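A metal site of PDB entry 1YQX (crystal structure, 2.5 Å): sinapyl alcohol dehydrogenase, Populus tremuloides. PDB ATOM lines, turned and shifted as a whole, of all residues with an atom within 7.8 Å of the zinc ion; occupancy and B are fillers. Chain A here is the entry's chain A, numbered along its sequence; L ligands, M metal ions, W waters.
The zinc ion is bound by SG of Cys 54, SG of Cys 170 and NE2 of His 76. The zinc ion has three donor atoms within binding distance. Slightly farther from the zinc ion lies water W1 (2.6 Å).
Merely in contact with the zinc ion: Ser 56. Within 4 Å of the zinc ion: Cys 54, Ser 56, His 76 and Cys 170. The nearest printed residue that does not touch the zinc ion is Glu 77 (4.8 Å).
SG of Cys 54 sits close to N of Ser 56 (3.5 Å). SG of Cys 54 sits close to NH2 of Arg 352 (3.6 Å). N of Cys 54 lies within hydrogen-bond range of OD1 of Asp 57. O of Cys 170 is in hydrogen-bond range of OG1 of Thr 174 (2.7 Å). ND1 of His 76 sits at hydrogen-bond distance from SG of Cys 102 (3.2 Å). O of Ser 56 is in hydrogen-bond range of OH of Tyr 128, 3.0 Å away.
O13 of the ligand is in hydrogen-bond range of OG of Ser 56 (2.7 Å). NH1 of Arg 352 is in salt-bridge range of O9 of the ligand (2.9 Å). The backbone NH (N) of His 55 sits at hydrogen-bond distance from an oxygen (O9) of the ligand, 2.9 Å away. An oxygen (O1) of the ligand sits at hydrogen-bond distance from a ring nitrogen (ND1) of His 55, 2.7 Å away. The backbone NH of Leu 199 lies within hydrogen-bond range of an oxygen (O8) of the ligand. The backbone NH of Ile 307 lies within hydrogen-bond range of an oxygen (O14) of the ligand (2.6 Å). An oxygen (O14) of the ligand sits close to the side-chain hydroxyl (OG1) of Thr 174 (3.5 Å).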
ATOM      1  N   GLY A  52      26.675   2.969 -25.646  1.00  0.00           N
ATOM      2  CA  GLY A  52      26.247   3.145 -24.272  1.00  0.00           C
ATOM      3  C   GLY A  52      25.133   4.154 -24.143  1.00  0.00           C
ATOM      4  O   GLY A  52      25.015   5.063 -24.979  1.00  0.00           O
ATOM      5  N   VAL A  53      24.311   4.004 -23.106  1.00  0.00           N
ATOM      6  CA  VAL A  53      23.214   4.915 -22.875  1.00  0.00           C
ATOM      7  C   VAL A  53      23.620   5.880 -21.782  1.00  0.00           C
ATOM      8  O   VAL A  53      23.810   5.488 -20.626  1.00  0.00           O
ATOM      9  CB  VAL A  53      21.926   4.168 -22.486  1.00  0.00           C
ATOM     10  CG1 VAL A  53      20.892   5.143 -21.926  1.00  0.00           C
ATOM     11  CG2 VAL A  53      21.380   3.452 -23.721  1.00  0.00           C
ATOM     12  N   CYS A  54      23.757   7.144 -22.177  1.00  0.00           N
ATOM     13  CA  CYS A  54      24.174   8.203 -21.276  1.00  0.00           C
ATOM     14  C   CYS A  54      22.941   8.952 -20.792  1.00  0.00           C
ATOM     15  O   CYS A  54      21.948   9.031 -21.509  1.00  0.00           O
ATOM     16  CB  CYS A  54      25.125   9.157 -22.012  1.00  0.00           C
ATOM     17  SG  CYS A  54      25.698  10.583 -21.042  1.00  0.00           S
ATOM     18  N   HIS A  55      23.006   9.511 -19.582  1.00  0.00           N
ATOM     19  CA  HIS A  55      21.853  10.241 -19.064  1.00  0.00           C
ATOM     20  C   HIS A  55      21.533  11.467 -19.931  1.00  0.00           C
ATOM     21  O   HIS A  55      20.440  12.000 -19.871  1.00  0.00           O
ATOM     22  CB  HIS A  55      22.078  10.656 -17.615  1.00  0.00           C
ATOM     23  CG  HIS A  55      20.818  10.949 -16.858  1.00  0.00           C
ATOM     24  ND1 HIS A  55      20.379  10.171 -15.806  1.00  0.00           N
ATOM     25  CD2 HIS A  55      19.923  11.956 -16.971  1.00  0.00           C
ATOM     26  CE1 HIS A  55      19.281  10.696 -15.296  1.00  0.00           C
ATOM     27  NE2 HIS A  55      18.984  11.774 -15.984  1.00  0.00           N
ATOM     28  N   SER A  56      22.499  11.884 -20.748  1.00  0.00           N
ATOM     29  CA  SER A  56      22.300  13.029 -21.646  1.00  0.00           C
ATOM     30  C   SER A  56      21.317  12.661 -22.744  1.00  0.00           C
ATOM     31  O   SER A  56      20.620  13.513 -23.271  1.00  0.00           O
ATOM     32  CB  SER A  56      23.620  13.458 -22.283  1.00  0.00           C
ATOM     33  OG  SER A  56      24.390  14.213 -21.369  1.00  0.00           O
ATOM     34  N   ASP A  57      21.273  11.390 -23.109  1.00  0.00           N
ATOM     35  CA  ASP A  57      20.343  10.910 -24.123  1.00  0.00           C
ATOM     36  C   ASP A  57      18.941  11.064 -23.530  1.00  0.00           C
ATOM     37  O   ASP A  57      17.998  11.404 -24.241  1.00  0.00           O
ATOM     38  CB  ASP A  57      20.607   9.433 -24.435  1.00  0.00           C
ATOM     39  CG  ASP A  57      21.985   9.199 -25.021  1.00  0.00           C
ATOM     40  OD1 ASP A  57      22.517   8.083 -24.844  1.00  0.00           O
ATOM     41  OD2 ASP A  57      22.519  10.109 -25.678  1.00  0.00           O
ATOM     42  N   TRP A  65      16.386  20.417 -21.300  1.00  0.00           N
ATOM     43  CA  TRP A  65      17.071  21.686 -21.439  1.00  0.00           C
ATOM     44  C   TRP A  65      16.385  22.627 -22.417  1.00  0.00           C
ATOM     45  O   TRP A  65      16.808  23.771 -22.577  1.00  0.00           O
ATOM     46  CB  TRP A  65      18.521  21.454 -21.857  1.00  0.00           C
ATOM     47  CG  TRP A  65      19.273  20.571 -20.882  1.00  0.00           C
ATOM     48  CD1 TRP A  65      19.289  20.697 -19.531  1.00  0.00           C
ATOM     49  CD2 TRP A  65      20.108  19.456 -21.198  1.00  0.00           C
ATOM     50  NE1 TRP A  65      20.079  19.715 -18.969  1.00  0.00           N
ATOM     51  CE2 TRP A  65      20.595  18.940 -19.975  1.00  0.00           C
ATOM     52  CE3 TRP A  65      20.497  18.832 -22.389  1.00  0.00           C
ATOM     53  CZ2 TRP A  65      21.452  17.838 -19.903  1.00  0.00           C
ATOM     54  CZ3 TRP A  65      21.352  17.728 -22.327  1.00  0.00           C
ATOM     55  CH2 TRP A  65      21.823  17.245 -21.094  1.00  0.00           C
ATOM     56  N   GLY A  75      22.466   8.856 -28.683  1.00  0.00           N
ATOM     57  CA  GLY A  75      23.619   7.983 -28.777  1.00  0.00           C
ATOM     58  C   GLY A  75      24.940   8.622 -29.130  1.00  0.00           C
ATOM     59  O   GLY A  75      25.164   9.011 -30.275  1.00  0.00           O
ATOM     60  N   HIS A  76      25.842   8.743 -28.167  1.00  0.00           N
ATOM     61  CA  HIS A  76      27.150   9.315 -28.424  1.00  0.00           C
ATOM     62  C   HIS A  76      28.260   8.624 -27.647  1.00  0.00           C
ATOM     63  O   HIS A  76      29.219   9.258 -27.191  1.00  0.00           O
ATOM     64  CB  HIS A  76      27.143  10.836 -28.172  1.00  0.00           C
ATOM     65  CG  HIS A  76      26.733  11.224 -26.789  1.00  0.00           C
ATOM     66  ND1 HIS A  76      26.465  12.534 -26.444  1.00  0.00           N
ATOM     67  CD2 HIS A  76      26.518  10.487 -25.673  1.00  0.00           C
ATOM     68  CE1 HIS A  76      26.096  12.583 -25.172  1.00  0.00           C
ATOM     69  NE2 HIS A  76      26.127  11.355 -24.689  1.00  0.00           N
ATOM     70  N   GLU A  77      28.102   7.308 -27.490  1.00  0.00           N
ATOM     71  CA  GLU A  77      29.064   6.424 -26.838  1.00  0.00           C
ATOM     72  C   GLU A  77      29.058   5.251 -27.797  1.00  0.00           C
ATOM     73  O   GLU A  77      28.791   4.101 -27.415  1.00  0.00           O
ATOM     74  CB  GLU A  77      28.562   5.967 -25.458  1.00  0.00           C
ATOM     75  CG  GLU A  77      28.735   7.030 -24.371  1.00  0.00           C
ATOM     76  CD  GLU A  77      28.443   6.528 -22.965  1.00  0.00           C
ATOM     77  OE1 GLU A  77      28.767   7.255 -22.007  1.00  0.00           O
ATOM     78  OE2 GLU A  77      27.885   5.428 -22.817  1.00  0.00           O
ATOM     79  N   GLY A 101      32.502   9.674 -30.024  1.00  0.00           N
ATOM     80  CA  GLY A 101      31.973  10.199 -28.785  1.00  0.00           C
ATOM     81  C   GLY A 101      30.865  11.230 -28.930  1.00  0.00           C
ATOM     82  O   GLY A 101      29.951  11.053 -29.717  1.00  0.00           O
ATOM     83  N   CYS A 102      30.973  12.302 -28.161  1.00  0.00           N
ATOM     84  CA  CYS A 102      29.975  13.359 -28.161  1.00  0.00           C
ATOM     85  C   CYS A 102      30.272  14.446 -29.207  1.00  0.00           C
ATOM     86  O   CYS A 102      29.438  15.306 -29.493  1.00  0.00           O
ATOM     87  CB  CYS A 102      29.894  13.951 -26.751  1.00  0.00           C
ATOM     88  SG  CYS A 102      28.495  15.059 -26.418  1.00  0.00           S
ATOM     89  N   TYR A 128      24.857  14.331 -31.769  1.00  0.00           N
ATOM     90  CA  TYR A 128      23.436  14.250 -32.077  1.00  0.00           C
ATOM     91  C   TYR A 128      22.703  15.510 -31.639  1.00  0.00           C
ATOM     92  O   TYR A 128      23.186  16.255 -30.797  1.00  0.00           O
ATOM     93  CB  TYR A 128      22.805  13.000 -31.424  1.00  0.00           C
ATOM     94  CG  TYR A 128      22.627  13.063 -29.922  1.00  0.00           C
ATOM     95  CD1 TYR A 128      21.634  13.865 -29.360  1.00  0.00           C
ATOM     96  CD2 TYR A 128      23.465  12.353 -29.064  1.00  0.00           C
ATOM     97  CE1 TYR A 128      21.479  13.950 -27.981  1.00  0.00           C
ATOM     98  CE2 TYR A 128      23.330  12.437 -27.690  1.00  0.00           C
ATOM     99  CZ  TYR A 128      22.330  13.235 -27.157  1.00  0.00           C
ATOM    100  OH  TYR A 128      22.196  13.359 -25.788  1.00  0.00           O
ATOM    101  N   PRO A 167      31.054   3.253 -22.939  1.00  0.00           N
ATOM    102  CA  PRO A 167      30.770   4.438 -22.116  1.00  0.00           C
ATOM    103  C   PRO A 167      31.965   5.314 -21.823  1.00  0.00           C
ATOM    104  O   PRO A 167      31.821   6.488 -21.481  1.00  0.00           O
ATOM    105  CB  PRO A 167      30.115   3.839 -20.856  1.00  0.00           C
ATOM    106  CG  PRO A 167      30.574   2.439 -20.852  1.00  0.00           C
ATOM    107  CD  PRO A 167      30.558   2.038 -22.293  1.00  0.00           C
ATOM    108  N   LEU A 169      33.819   6.545 -23.893  1.00  0.00           N
ATOM    109  CA  LEU A 169      33.812   7.596 -24.910  1.00  0.00           C
ATOM    110  C   LEU A 169      33.218   8.918 -24.423  1.00  0.00           C
ATOM    111  O   LEU A 169      33.587   9.988 -24.913  1.00  0.00           O
ATOM    112  CB  LEU A 169      33.076   7.128 -26.151  1.00  0.00           C
ATOM    113  CG  LEU A 169      33.802   6.025 -26.918  1.00  0.00           C
ATOM    114  CD1 LEU A 169      32.911   5.512 -28.020  1.00  0.00           C
ATOM    115  CD2 LEU A 169      35.115   6.555 -27.483  1.00  0.00           C
ATOM    116  N   CYS A 170      32.289   8.861 -23.475  1.00  0.00           N
ATOM    117  CA  CYS A 170      31.727  10.095 -22.963  1.00  0.00           C
ATOM    118  C   CYS A 170      31.832  10.150 -21.438  1.00  0.00           C
ATOM    119  O   CYS A 170      32.464  11.053 -20.882  1.00  0.00           O
ATOM    120  CB  CYS A 170      30.268  10.235 -23.362  1.00  0.00           C
ATOM    121  SG  CYS A 170      29.520  11.736 -22.713  1.00  0.00           S
ATOM    122  N   ALA A 171      31.223   9.174 -20.774  1.00  0.00           N
ATOM    123  CA  ALA A 171      31.252   9.122 -19.319  1.00  0.00           C
ATOM    124  C   ALA A 171      32.704   9.141 -18.866  1.00  0.00           C
ATOM    125  O   ALA A 171      33.079   9.898 -17.967  1.00  0.00           O
ATOM    126  CB  ALA A 171      30.570   7.851 -18.828  1.00  0.00           C
ATOM    127  N   THR A 174      34.811  12.300 -19.856  1.00  0.00           N
ATOM    128  CA  THR A 174      34.262  13.407 -19.082  1.00  0.00           C
ATOM    129  C   THR A 174      34.735  13.539 -17.638  1.00  0.00           C
ATOM    130  O   THR A 174      34.870  14.653 -17.151  1.00  0.00           O
ATOM    131  CB  THR A 174      32.706  13.374 -19.154  1.00  0.00           C
ATOM    132  OG1 THR A 174      32.296  13.731 -20.479  1.00  0.00           O
ATOM    133  CG2 THR A 174      32.077  14.372 -18.168  1.00  0.00           C
ATOM    134  N   LEU A 199      28.747   8.116 -15.067  1.00  0.00           N
ATOM    135  CA  LEU A 199      29.984   8.865 -14.946  1.00  0.00           C
ATOM    136  C   LEU A 199      30.655   8.633 -13.598  1.00  0.00           C
ATOM    137  O   LEU A 199      31.873   8.498 -13.513  1.00  0.00           O
ATOM    138  CB  LEU A 199      29.731  10.371 -15.149  1.00  0.00           C
ATOM    139  CG  LEU A 199      29.793  10.854 -16.609  1.00  0.00           C
ATOM    140  CD1 LEU A 199      28.640  10.251 -17.405  1.00  0.00           C
ATOM    141  CD2 LEU A 199      29.742  12.383 -16.669  1.00  0.00           C
ATOM    142  N   ILE A 307      33.008  16.907 -21.359  1.00  0.00           N
ATOM    143  CA  ILE A 307      33.763  15.871 -22.070  1.00  0.00           C
ATOM    144  C   ILE A 307      35.242  16.209 -22.153  1.00  0.00           C
ATOM    145  O   ILE A 307      35.869  16.585 -21.164  1.00  0.00           O
ATOM    146  CB  ILE A 307      33.225  15.671 -23.509  1.00  0.00           C
ATOM    147  CG1 ILE A 307      33.137  17.030 -24.224  1.00  0.00           C
ATOM    148  CG2 ILE A 307      31.874  14.978 -23.475  1.00  0.00           C
ATOM    149  CD1 ILE A 307      32.629  16.942 -25.654  1.00  0.00           C
ATOM    150  N   ARG A 352      25.774   1.062 -16.173  1.00  0.00           N
ATOM    151  CA  ARG A 352      25.564   1.569 -17.526  1.00  0.00           C
ATOM    152  C   ARG A 352      24.886   0.647 -18.525  1.00  0.00           C
ATOM    153  O   ARG A 352      25.290  -0.488 -18.740  1.00  0.00           O
ATOM    154  CB  ARG A 352      26.910   2.044 -18.113  1.00  0.00           C
ATOM    155  CG  ARG A 352      27.089   3.551 -18.197  1.00  0.00           C
ATOM    156  CD  ARG A 352      26.454   4.128 -19.452  1.00  0.00           C
ATOM    157  NE  ARG A 352      26.958   5.465 -19.804  1.00  0.00           N
ATOM    158  CZ  ARG A 352      26.706   6.579 -19.125  1.00  0.00           C
ATOM    159  NH1 ARG A 352      25.947   6.555 -18.038  1.00  0.00           N
ATOM    160  NH2 ARG A 352      27.210   7.724 -19.546  1.00  0.00           N
HETATM  161  P1  LIG L   1      23.123   8.429 -14.234  1.00  0.00           P
HETATM  162  O1  LIG L   1      21.765   8.628 -14.105  1.00  0.00           O
HETATM  163  O2  LIG L   1      23.769   7.160 -14.689  1.00  0.00           O
HETATM  164  O3  LIG L   1      23.907   8.768 -12.885  1.00  0.00           O
HETATM  165  C1  LIG L   1      23.502   9.952 -12.177  1.00  0.00           C
HETATM  166  C2  LIG L   1      23.944   9.494 -10.774  1.00  0.00           C
HETATM  167  O4  LIG L   1      23.510  10.667  -9.715  1.00  0.00           O
HETATM  168  C3  LIG L   1      22.687   8.621 -10.044  1.00  0.00           C
HETATM  169  O5  LIG L   1      23.389   7.278  -9.995  1.00  0.00           O
HETATM  170  C4  LIG L   1      22.579   8.923  -8.622  1.00  0.00           C
HETATM  171  O6  LIG L   1      23.735   8.579  -7.881  1.00  0.00           O
HETATM  172  C5  LIG L   1      22.744  10.516  -8.744  1.00  0.00           C
HETATM  173  N1  LIG L   1      21.415  11.150  -8.752  1.00  0.00           N
HETATM  174  C6  LIG L   1      20.338  11.028  -9.629  1.00  0.00           C
HETATM  175  N2  LIG L   1      19.289  11.791  -9.287  1.00  0.00           N
HETATM  176  C7  LIG L   1      19.721  12.432  -8.117  1.00  0.00           C
HETATM  177  C8  LIG L   1      19.030  13.396  -7.247  1.00  0.00           C
HETATM  178  N3  LIG L   1      17.782  13.897  -7.393  1.00  0.00           N
HETATM  179  N4  LIG L   1      19.755  13.892  -6.101  1.00  0.00           N
HETATM  180  C9  LIG L   1      21.094  13.433  -5.848  1.00  0.00           C
HETATM  181  N5  LIG L   1      21.766  12.505  -6.677  1.00  0.00           N
HETATM  182  C10 LIG L   1      21.049  12.033  -7.797  1.00  0.00           C
HETATM  183  O7  LIG L   1      23.714   9.523 -15.220  1.00  0.00           O
HETATM  184  P2  LIG L   1      25.092   9.477 -15.987  1.00  0.00           P
HETATM  185  O8  LIG L   1      26.338   9.738 -15.305  1.00  0.00           O
HETATM  186  O9  LIG L   1      24.968   9.244 -17.412  1.00  0.00           O
HETATM  187  O10 LIG L   1      24.951  11.089 -16.274  1.00  0.00           O
HETATM  188  C11 LIG L   1      24.977  12.108 -15.186  1.00  0.00           C
HETATM  189  C12 LIG L   1      24.865  13.573 -15.648  1.00  0.00           C
HETATM  190  O11 LIG L   1      26.068  14.073 -16.317  1.00  0.00           O
HETATM  191  C13 LIG L   1      23.702  14.012 -16.659  1.00  0.00           C
HETATM  192  O12 LIG L   1      23.110  15.284 -16.238  1.00  0.00           O
HETATM  193  C14 LIG L   1      24.415  14.147 -17.968  1.00  0.00           C
HETATM  194  O13 LIG L   1      23.667  14.925 -18.899  1.00  0.00           O
HETATM  195  C15 LIG L   1      25.663  14.765 -17.552  1.00  0.00           C
HETATM  196  N6  LIG L   1      26.839  14.673 -18.417  1.00  0.00           N
HETATM  197  C16 LIG L   1      27.668  15.812 -18.648  1.00  0.00           C
HETATM  198  C17 LIG L   1      28.787  15.685 -19.485  1.00  0.00           C
HETATM  199  C18 LIG L   1      29.655  16.916 -19.706  1.00  0.00           C
HETATM  200  O14 LIG L   1      30.616  16.790 -20.431  1.00  0.00           O
HETATM  201  N7  LIG L   1      29.358  18.047 -19.133  1.00  0.00           N
HETATM  202  C19 LIG L   1      29.139  14.402 -20.125  1.00  0.00           C
HETATM  203  C20 LIG L   1      28.277  13.287 -19.868  1.00  0.00           C
HETATM  204  C21 LIG L   1      27.111  13.389 -19.006  1.00  0.00           C
HETATM  205  P3  LIG L   1      23.578   8.028  -6.284  1.00  0.00           P
HETATM  206  O15 LIG L   1      25.024   7.741  -5.852  1.00  0.00           O
HETATM  207  O16 LIG L   1      22.946   9.191  -5.569  1.00  0.00           O
HETATM  208  O17 LIG L   1      22.770   6.755  -6.353  1.00  0.00           O
HETATM  209 ZN    ZN M   1      27.132  11.768 -22.532  1.00  0.00          ZN
HETATM  210  O   HOH W   1      26.867  14.397 -22.733  1.00  0.00           O
